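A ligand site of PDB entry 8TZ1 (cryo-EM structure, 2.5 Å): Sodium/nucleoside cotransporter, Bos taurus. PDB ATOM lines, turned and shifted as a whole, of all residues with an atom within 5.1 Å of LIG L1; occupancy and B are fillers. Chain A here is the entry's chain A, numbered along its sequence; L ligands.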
ATOM      1  N   TRP A 191     -38.181 -15.710   2.906  1.00  0.00           N
ATOM      2  CA  TRP A 191     -37.444 -15.670   4.164  1.00  0.00           C
ATOM      3  C   TRP A 191     -37.603 -16.952   4.962  1.00  0.00           C
ATOM      4  O   TRP A 191     -36.696 -17.328   5.717  1.00  0.00           O
ATOM      5  CB  TRP A 191     -37.894 -14.472   4.998  1.00  0.00           C
ATOM      6  CG  TRP A 191     -37.417 -14.512   6.418  1.00  0.00           C
ATOM      7  CD1 TRP A 191     -38.145 -14.863   7.517  1.00  0.00           C
ATOM      8  CD2 TRP A 191     -36.107 -14.189   6.885  1.00  0.00           C
ATOM      9  NE1 TRP A 191     -37.368 -14.778   8.646  1.00  0.00           N
ATOM     10  CE2 TRP A 191     -36.112 -14.366   8.282  1.00  0.00           C
ATOM     11  CE3 TRP A 191     -34.936 -13.764   6.270  1.00  0.00           C
ATOM     12  CZ2 TRP A 191     -34.984 -14.138   9.074  1.00  0.00           C
ATOM     13  CZ3 TRP A 191     -33.818 -13.534   7.049  1.00  0.00           C
ATOM     14  CH2 TRP A 191     -33.852 -13.719   8.437  1.00  0.00           C
ATOM     15  N   ILE A 198     -28.790 -17.775   5.808  1.00  0.00           N
ATOM     16  CA  ILE A 198     -28.098 -16.586   6.299  1.00  0.00           C
ATOM     17  C   ILE A 198     -27.495 -16.848   7.678  1.00  0.00           C
ATOM     18  O   ILE A 198     -26.342 -16.497   7.953  1.00  0.00           O
ATOM     19  CB  ILE A 198     -29.058 -15.384   6.317  1.00  0.00           C
ATOM     20  CG1 ILE A 198     -29.495 -15.039   4.890  1.00  0.00           C
ATOM     21  CG2 ILE A 198     -28.392 -14.175   6.976  1.00  0.00           C
ATOM     22  CD1 ILE A 198     -30.506 -13.930   4.798  1.00  0.00           C
ATOM     23  N   TRP A 199     -28.281 -17.455   8.562  1.00  0.00           N
ATOM     24  CA  TRP A 199     -27.775 -17.747   9.905  1.00  0.00           C
ATOM     25  C   TRP A 199     -26.600 -18.699   9.860  1.00  0.00           C
ATOM     26  O   TRP A 199     -25.608 -18.518  10.579  1.00  0.00           O
ATOM     27  CB  TRP A 199     -28.905 -18.304  10.778  1.00  0.00           C
ATOM     28  CG  TRP A 199     -30.006 -17.328  11.022  1.00  0.00           C
ATOM     29  CD1 TRP A 199     -30.006 -15.992  10.753  1.00  0.00           C
ATOM     30  CD2 TRP A 199     -31.295 -17.621  11.570  1.00  0.00           C
ATOM     31  NE1 TRP A 199     -31.204 -15.429  11.114  1.00  0.00           N
ATOM     32  CE2 TRP A 199     -32.016 -16.408  11.622  1.00  0.00           C
ATOM     33  CE3 TRP A 199     -31.914 -18.781  12.037  1.00  0.00           C
ATOM     34  CZ2 TRP A 199     -33.317 -16.334  12.116  1.00  0.00           C
ATOM     35  CZ3 TRP A 199     -33.204 -18.706  12.532  1.00  0.00           C
ATOM     36  CH2 TRP A 199     -33.885 -17.486  12.556  1.00  0.00           C
ATOM     37  N   LEU A 202     -23.453 -16.862   8.769  1.00  0.00           N
ATOM     38  CA  LEU A 202     -22.923 -16.021   9.832  1.00  0.00           C
ATOM     39  C   LEU A 202     -22.205 -16.855  10.889  1.00  0.00           C
ATOM     40  O   LEU A 202     -21.118 -16.482  11.354  1.00  0.00           O
ATOM     41  CB  LEU A 202     -24.045 -15.205  10.472  1.00  0.00           C
ATOM     42  CG  LEU A 202     -24.673 -14.128   9.592  1.00  0.00           C
ATOM     43  CD1 LEU A 202     -25.964 -13.635  10.205  1.00  0.00           C
ATOM     44  CD2 LEU A 202     -23.711 -12.967   9.396  1.00  0.00           C
ATOM     45  N   GLY A 205     -18.929 -17.957   9.476  1.00  0.00           N
ATOM     46  CA  GLY A 205     -17.967 -16.864   9.476  1.00  0.00           C
ATOM     47  C   GLY A 205     -17.356 -16.634  10.835  1.00  0.00           C
ATOM     48  O   GLY A 205     -16.151 -16.399  10.963  1.00  0.00           O
ATOM     49  N   VAL A 206     -18.171 -16.697  11.894  1.00  0.00           N
ATOM     50  CA  VAL A 206     -17.666 -16.523  13.248  1.00  0.00           C
ATOM     51  C   VAL A 206     -16.662 -17.613  13.573  1.00  0.00           C
ATOM     52  O   VAL A 206     -15.591 -17.354  14.155  1.00  0.00           O
ATOM     53  CB  VAL A 206     -18.826 -16.502  14.259  1.00  0.00           C
ATOM     54  CG1 VAL A 206     -18.299 -16.553  15.678  1.00  0.00           C
ATOM     55  CG2 VAL A 206     -19.674 -15.257  14.056  1.00  0.00           C
ATOM     56  N   TRP A 209     -13.356 -16.991  11.726  1.00  0.00           N
ATOM     57  CA  TRP A 209     -12.590 -15.898  12.304  1.00  0.00           C
ATOM     58  C   TRP A 209     -11.862 -16.347  13.567  1.00  0.00           C
ATOM     59  O   TRP A 209     -10.685 -16.026  13.766  1.00  0.00           O
ATOM     60  CB  TRP A 209     -13.506 -14.716  12.598  1.00  0.00           C
ATOM     61  CG  TRP A 209     -12.775 -13.539  13.174  1.00  0.00           C
ATOM     62  CD1 TRP A 209     -12.629 -13.226  14.489  1.00  0.00           C
ATOM     63  CD2 TRP A 209     -12.070 -12.531  12.440  1.00  0.00           C
ATOM     64  NE1 TRP A 209     -11.884 -12.083  14.623  1.00  0.00           N
ATOM     65  CE2 TRP A 209     -11.530 -11.633  13.376  1.00  0.00           C
ATOM     66  CE3 TRP A 209     -11.849 -12.294  11.078  1.00  0.00           C
ATOM     67  CZ2 TRP A 209     -10.771 -10.522  13.004  1.00  0.00           C
ATOM     68  CZ3 TRP A 209     -11.098 -11.197  10.702  1.00  0.00           C
ATOM     69  CH2 TRP A 209     -10.579 -10.320  11.664  1.00  0.00           C
ATOM     70  N   TYR A 246     -36.691 -11.055  23.125  1.00  0.00           N
ATOM     71  CA  TYR A 246     -36.619 -10.816  21.689  1.00  0.00           C
ATOM     72  C   TYR A 246     -35.140 -10.741  21.323  1.00  0.00           C
ATOM     73  O   TYR A 246     -34.450  -9.780  21.670  1.00  0.00           O
ATOM     74  CB  TYR A 246     -37.355  -9.525  21.338  1.00  0.00           C
ATOM     75  CG  TYR A 246     -37.418  -9.196  19.864  1.00  0.00           C
ATOM     76  CD1 TYR A 246     -37.630 -10.182  18.904  1.00  0.00           C
ATOM     77  CD2 TYR A 246     -37.312  -7.876  19.430  1.00  0.00           C
ATOM     78  CE1 TYR A 246     -37.696  -9.868  17.564  1.00  0.00           C
ATOM     79  CE2 TYR A 246     -37.378  -7.562  18.090  1.00  0.00           C
ATOM     80  CZ  TYR A 246     -37.570  -8.551  17.159  1.00  0.00           C
ATOM     81  OH  TYR A 246     -37.636  -8.237  15.819  1.00  0.00           O
ATOM     82  N   ARG A 248     -33.446 -10.532  18.460  1.00  0.00           N
ATOM     83  CA  ARG A 248     -32.909  -9.720  17.361  1.00  0.00           C
ATOM     84  C   ARG A 248     -32.022  -8.597  17.852  1.00  0.00           C
ATOM     85  O   ARG A 248     -30.884  -8.475  17.366  1.00  0.00           O
ATOM     86  CB  ARG A 248     -34.063  -9.194  16.505  1.00  0.00           C
ATOM     87  CG  ARG A 248     -33.652  -8.283  15.363  1.00  0.00           C
ATOM     88  CD  ARG A 248     -34.864  -7.595  14.770  1.00  0.00           C
ATOM     89  NE  ARG A 248     -34.522  -6.704  13.674  1.00  0.00           N
ATOM     90  CZ  ARG A 248     -35.365  -5.846  13.121  1.00  0.00           C
ATOM     91  NH1 ARG A 248     -36.616  -5.735  13.542  1.00  0.00           N
ATOM     92  NH2 ARG A 248     -34.947  -5.086  12.112  1.00  0.00           N
ATOM     93  N   PHE A 251     -28.355  -9.900  19.250  1.00  0.00           N
ATOM     94  CA  PHE A 251     -27.361 -10.312  18.273  1.00  0.00           C
ATOM     95  C   PHE A 251     -26.903  -9.143  17.418  1.00  0.00           C
ATOM     96  O   PHE A 251     -25.711  -9.011  17.114  1.00  0.00           O
ATOM     97  CB  PHE A 251     -27.937 -11.421  17.388  1.00  0.00           C
ATOM     98  CG  PHE A 251     -28.153 -12.718  18.118  1.00  0.00           C
ATOM     99  CD1 PHE A 251     -27.179 -13.234  18.966  1.00  0.00           C
ATOM    100  CD2 PHE A 251     -29.326 -13.425  17.949  1.00  0.00           C
ATOM    101  CE1 PHE A 251     -27.390 -14.419  19.629  1.00  0.00           C
ATOM    102  CE2 PHE A 251     -29.537 -14.618  18.617  1.00  0.00           C
ATOM    103  CZ  PHE A 251     -28.564 -15.117  19.453  1.00  0.00           C
ATOM    104  N   TRP A 252     -27.831  -8.266  17.017  1.00  0.00           N
ATOM    105  CA  TRP A 252     -27.453  -7.123  16.200  1.00  0.00           C
ATOM    106  C   TRP A 252     -26.532  -6.177  16.957  1.00  0.00           C
ATOM    107  O   TRP A 252     -25.579  -5.639  16.393  1.00  0.00           O
ATOM    108  CB  TRP A 252     -28.701  -6.389  15.706  1.00  0.00           C
ATOM    109  CG  TRP A 252     -29.129  -6.814  14.340  1.00  0.00           C
ATOM    110  CD1 TRP A 252     -30.258  -7.523  14.028  1.00  0.00           C
ATOM    111  CD2 TRP A 252     -28.452  -6.568  13.115  1.00  0.00           C
ATOM    112  NE1 TRP A 252     -30.310  -7.723  12.676  1.00  0.00           N
ATOM    113  CE2 TRP A 252     -29.209  -7.157  12.090  1.00  0.00           C
ATOM    114  CE3 TRP A 252     -27.262  -5.920  12.774  1.00  0.00           C
ATOM    115  CZ2 TRP A 252     -28.827  -7.107  10.750  1.00  0.00           C
ATOM    116  CZ3 TRP A 252     -26.880  -5.866  11.456  1.00  0.00           C
ATOM    117  CH2 TRP A 252     -27.668  -6.454  10.452  1.00  0.00           C
ATOM    118  N   GLY A 255     -23.166  -7.728  17.055  1.00  0.00           N
ATOM    119  CA  GLY A 255     -22.582  -7.694  15.730  1.00  0.00           C
ATOM    120  C   GLY A 255     -22.101  -6.304  15.334  1.00  0.00           C
ATOM    121  O   GLY A 255     -21.042  -6.161  14.728  1.00  0.00           O
ATOM    122  N   LEU A 256     -22.878  -5.279  15.676  1.00  0.00           N
ATOM    123  CA  LEU A 256     -22.457  -3.912  15.355  1.00  0.00           C
ATOM    124  C   LEU A 256     -21.175  -3.556  16.092  1.00  0.00           C
ATOM    125  O   LEU A 256     -20.292  -2.894  15.533  1.00  0.00           O
ATOM    126  CB  LEU A 256     -23.572  -2.925  15.700  1.00  0.00           C
ATOM    127  CG  LEU A 256     -24.810  -2.959  14.808  1.00  0.00           C
ATOM    128  CD1 LEU A 256     -25.876  -2.039  15.365  1.00  0.00           C
ATOM    129  CD2 LEU A 256     -24.467  -2.566  13.380  1.00  0.00           C
ATOM    130  N   PHE A 258     -18.854  -5.693  16.967  1.00  0.00           N
ATOM    131  CA  PHE A 258     -17.786  -6.446  16.315  1.00  0.00           C
ATOM    132  C   PHE A 258     -17.356  -5.768  15.021  1.00  0.00           C
ATOM    133  O   PHE A 258     -16.150  -5.688  14.730  1.00  0.00           O
ATOM    134  CB  PHE A 258     -18.249  -7.873  16.060  1.00  0.00           C
ATOM    135  CG  PHE A 258     -17.164  -8.789  15.576  1.00  0.00           C
ATOM    136  CD1 PHE A 258     -16.130  -9.157  16.420  1.00  0.00           C
ATOM    137  CD2 PHE A 258     -17.189  -9.294  14.296  1.00  0.00           C
ATOM    138  CE1 PHE A 258     -15.132  -9.994  15.983  1.00  0.00           C
ATOM    139  CE2 PHE A 258     -16.190 -10.144  13.857  1.00  0.00           C
ATOM    140  CZ  PHE A 258     -15.167 -10.491  14.697  1.00  0.00           C
ATOM    141  N   LEU A 259     -18.308  -5.296  14.231  1.00  0.00           N
ATOM    142  CA  LEU A 259     -17.969  -4.611  12.987  1.00  0.00           C
ATOM    143  C   LEU A 259     -17.229  -3.305  13.262  1.00  0.00           C
ATOM    144  O   LEU A 259     -16.250  -2.983  12.585  1.00  0.00           O
ATOM    145  CB  LEU A 259     -19.228  -4.354  12.157  1.00  0.00           C
ATOM    146  CG  LEU A 259     -19.977  -5.593  11.685  1.00  0.00           C
ATOM    147  CD1 LEU A 259     -21.206  -5.191  10.901  1.00  0.00           C
ATOM    148  CD2 LEU A 259     -19.085  -6.495  10.856  1.00  0.00           C
ATOM    149  N   LEU A 262     -13.693  -4.115  14.223  1.00  0.00           N
ATOM    150  CA  LEU A 262     -12.904  -4.532  13.063  1.00  0.00           C
ATOM    151  C   LEU A 262     -12.479  -3.326  12.228  1.00  0.00           C
ATOM    152  O   LEU A 262     -11.321  -3.240  11.794  1.00  0.00           O
ATOM    153  CB  LEU A 262     -13.690  -5.518  12.209  1.00  0.00           C
ATOM    154  CG  LEU A 262     -13.810  -6.956  12.703  1.00  0.00           C
ATOM    155  CD1 LEU A 262     -14.583  -7.779  11.696  1.00  0.00           C
ATOM    156  CD2 LEU A 262     -12.444  -7.559  12.926  1.00  0.00           C
HETATM  157  C1  LIG L   1     -35.484 -11.000  11.250  1.00  0.00           C
HETATM  158  P1  LIG L   1     -37.534 -10.305  12.773  1.00  0.00           P
HETATM  159  C2  LIG L   1     -33.986 -11.176  11.509  1.00  0.00           C
HETATM  160  C3  LIG L   1     -33.179 -10.164  10.706  1.00  0.00           C
HETATM  161  C4  LIG L   1     -22.973  -8.878  12.470  1.00  0.00           C
HETATM  162  O1  LIG L   1     -36.010 -10.047  12.143  1.00  0.00           O
HETATM  163  C5  LIG L   1     -22.382 -10.165  11.845  1.00  0.00           C
HETATM  164  O2  LIG L   1     -37.433 -11.123  14.045  1.00  0.00           O
HETATM  165  C6  LIG L   1     -20.842 -10.174  12.025  1.00  0.00           C
HETATM  166  O3  LIG L   1     -38.188  -8.984  13.072  1.00  0.00           O
HETATM  167  C7  LIG L   1     -20.242 -11.469  11.457  1.00  0.00           C
HETATM  168  O4  LIG L   1     -38.444 -11.129  11.671  1.00  0.00           O
HETATM  169  C8  LIG L   1     -18.730 -11.533  11.649  1.00  0.00           C
HETATM  170  C9  LIG L   1     -18.121 -12.769  10.990  1.00  0.00           C
HETATM  171  C10 LIG L   1     -16.619 -12.836  11.195  1.00  0.00           C
HETATM  172  C11 LIG L   1     -15.812 -11.818  10.400  1.00  0.00           C
HETATM  173  C12 LIG L   1     -16.113 -11.841   8.915  1.00  0.00           C
HETATM  174  C13 LIG L   1     -31.429 -11.151   9.482  1.00  0.00           C
HETATM  175  O5  LIG L   1     -32.787 -10.775   9.508  1.00  0.00           O
HETATM  176  C14 LIG L   1     -30.340 -10.090   9.292  1.00  0.00           C
HETATM  177  O6  LIG L   1     -31.128 -12.292   9.608  1.00  0.00           O
HETATM  178  C15 LIG L   1     -29.184 -10.561   8.394  1.00  0.00           C
HETATM  179  C16 LIG L   1     -27.996  -9.576   8.452  1.00  0.00           C
HETATM  180  C17 LIG L   1     -26.750 -10.086   7.700  1.00  0.00           C
HETATM  181  C18 LIG L   1     -25.475  -9.387   8.178  1.00  0.00           C
HETATM  182  C19 LIG L   1     -24.354  -9.404   7.124  1.00  0.00           C
HETATM  183  C20 LIG L   1     -33.492 -12.198  13.585  1.00  0.00           C
HETATM  184  O7  LIG L   1     -33.714 -10.972  12.887  1.00  0.00           O
HETATM  185  C21 LIG L   1     -32.062 -12.799  13.652  1.00  0.00           C
HETATM  186  O8  LIG L   1     -34.402 -12.762  14.110  1.00  0.00           O
HETATM  187  C22 LIG L   1     -30.986 -11.763  14.046  1.00  0.00           C
HETATM  188  C23 LIG L   1     -29.776 -11.822  13.116  1.00  0.00           C
HETATM  189  C24 LIG L   1     -28.531 -11.161  13.731  1.00  0.00           C
HETATM  190  C25 LIG L   1     -27.392 -11.012  12.719  1.00  0.00           C
HETATM  191  C26 LIG L   1     -26.337  -9.991  13.161  1.00  0.00           C
HETATM  192  C27 LIG L   1     -25.345  -9.672  12.017  1.00  0.00           C
HETATM  193  C28 LIG L   1     -24.302  -8.658  12.536  1.00  0.00           C
HETATM  194  C1  LG2 L   2     -36.511 -17.165  18.695  1.00  0.00           C
HETATM  195  P1  LG2 L   2     -37.315 -14.617  18.584  1.00  0.00           P
HETATM  196  C2  LG2 L   2     -35.030 -16.986  18.353  1.00  0.00           C
HETATM  197  C3  LG2 L   2     -34.225 -18.081  19.025  1.00  0.00           C
HETATM  198  C4  LG2 L   2     -24.535 -14.457  15.510  1.00  0.00           C
HETATM  199  O1  LG2 L   2     -37.279 -16.190  18.026  1.00  0.00           O
HETATM  200  C5  LG2 L   2     -24.607 -12.997  15.024  1.00  0.00           C
HETATM  201  O2  LG2 L   2     -36.146 -13.855  18.010  1.00  0.00           O
HETATM  202  C6  LG2 L   2     -23.756 -12.107  15.964  1.00  0.00           C
HETATM  203  O3  LG2 L   2     -37.225 -14.598  20.094  1.00  0.00           O
HETATM  204  C7  LG2 L   2     -22.271 -12.148  15.607  1.00  0.00           C
HETATM  205  O4  LG2 L   2     -38.722 -13.898  18.114  1.00  0.00           O
HETATM  206  C8  LG2 L   2     -21.415 -11.568  16.733  1.00  0.00           C
HETATM  207  C9  LG2 L   2     -19.970 -12.019  16.631  1.00  0.00           C
HETATM  208  C10 LG2 L   2     -19.149 -11.545  17.817  1.00  0.00           C
HETATM  209  C11 LG2 L   2     -17.741 -12.120  17.888  1.00  0.00           C
HETATM  210  C12 LG2 L   2     -17.288 -12.893  16.651  1.00  0.00           C
HETATM  211  C13 LG2 L   2     -32.357 -18.388  20.429  1.00  0.00           C
HETATM  212  O5  LG2 L   2     -33.232 -17.474  19.820  1.00  0.00           O
HETATM  213  C14 LG2 L   2     -30.938 -18.560  19.878  1.00  0.00           C
HETATM  214  O6  LG2 L   2     -32.711 -19.017  21.360  1.00  0.00           O
HETATM  215  C15 LG2 L   2     -29.851 -18.446  20.960  1.00  0.00           C
HETATM  216  C16 LG2 L   2     -28.596 -19.253  20.582  1.00  0.00           C
HETATM  217  C17 LG2 L   2     -28.108 -18.937  19.157  1.00  0.00           C
HETATM  218  C18 LG2 L   2     -26.577 -19.003  19.019  1.00  0.00           C
HETATM  219  C19 LG2 L   2     -26.124 -18.905  17.552  1.00  0.00           C
HETATM  220  C20 LG2 L   2     -33.988 -16.053  16.415  1.00  0.00           C
HETATM  221  O7  LG2 L   2     -34.828 -17.074  16.952  1.00  0.00           O
HETATM  222  C21 LG2 L   2     -32.444 -16.139  16.625  1.00  0.00           C
HETATM  223  O8  LG2 L   2     -34.464 -15.131  15.842  1.00  0.00           O
HETATM  224  C22 LG2 L   2     -31.806 -17.348  15.900  1.00  0.00           C
HETATM  225  C23 LG2 L   2     -30.266 -17.309  15.958  1.00  0.00           C
HETATM  226  C24 LG2 L   2     -29.639 -16.728  14.687  1.00  0.00           C
HETATM  227  C25 LG2 L   2     -28.227 -16.195  14.961  1.00  0.00           C
HETATM  228  C26 LG2 L   2     -27.331 -16.227  13.730  1.00  0.00           C
HETATM  229  C27 LG2 L   2     -26.252 -15.113  13.785  1.00  0.00           C
HETATM  230  C28 LG2 L   2     -25.290 -15.423  14.953  1.00  0.00           C
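An oxygen (O6) of LIG L1 sits at hydrogen-bond distance from the indole nitrogen (NE1) of Trp 199 (3.5 Å). NH1 of Arg 248 is in salt-bridge range of O3 of LIG L1. An oxygen (O3) of LIG L1 is in hydrogen-bond range of the side-chain hydroxyl (OH) of Tyr 246, 2.9 Å away.
Trp 191 touches LIG L1. CG2 of Ile 198 touches C15 of LIG L1, at 3.96 Å. CD1 of Leu 202 touches C25 of LIG L1, at 3.9 Å. Gly 205 touches LIG L1 (O to C10, 3.6 Å). CB of Trp 209 touches C10 of LIG L1, at 3.9 Å. Phe 251 touches LIG L1 (CB to C24, 3.7 Å). Trp 252 touches LIG L1 (CZ2 to C16, 3.5 Å). Gly 255 touches LIG L1. Phe 258 touches LIG L1 (CE2 to C8, 3.6 Å). Hydrophobic or aromatic side chains that line LIG L1: Trp 191, Ile 198, Leu 202, Trp 209, Tyr 246, Phe 251, Trp 252 and Phe 258. Within 4 Å of LIG L1: Trp 191, Ile 198, Trp 199, Leu 202, Gly 205, Trp 209, Tyr 246, Arg 248, Phe 251, Trp 252, Gly 255 and Phe 258.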
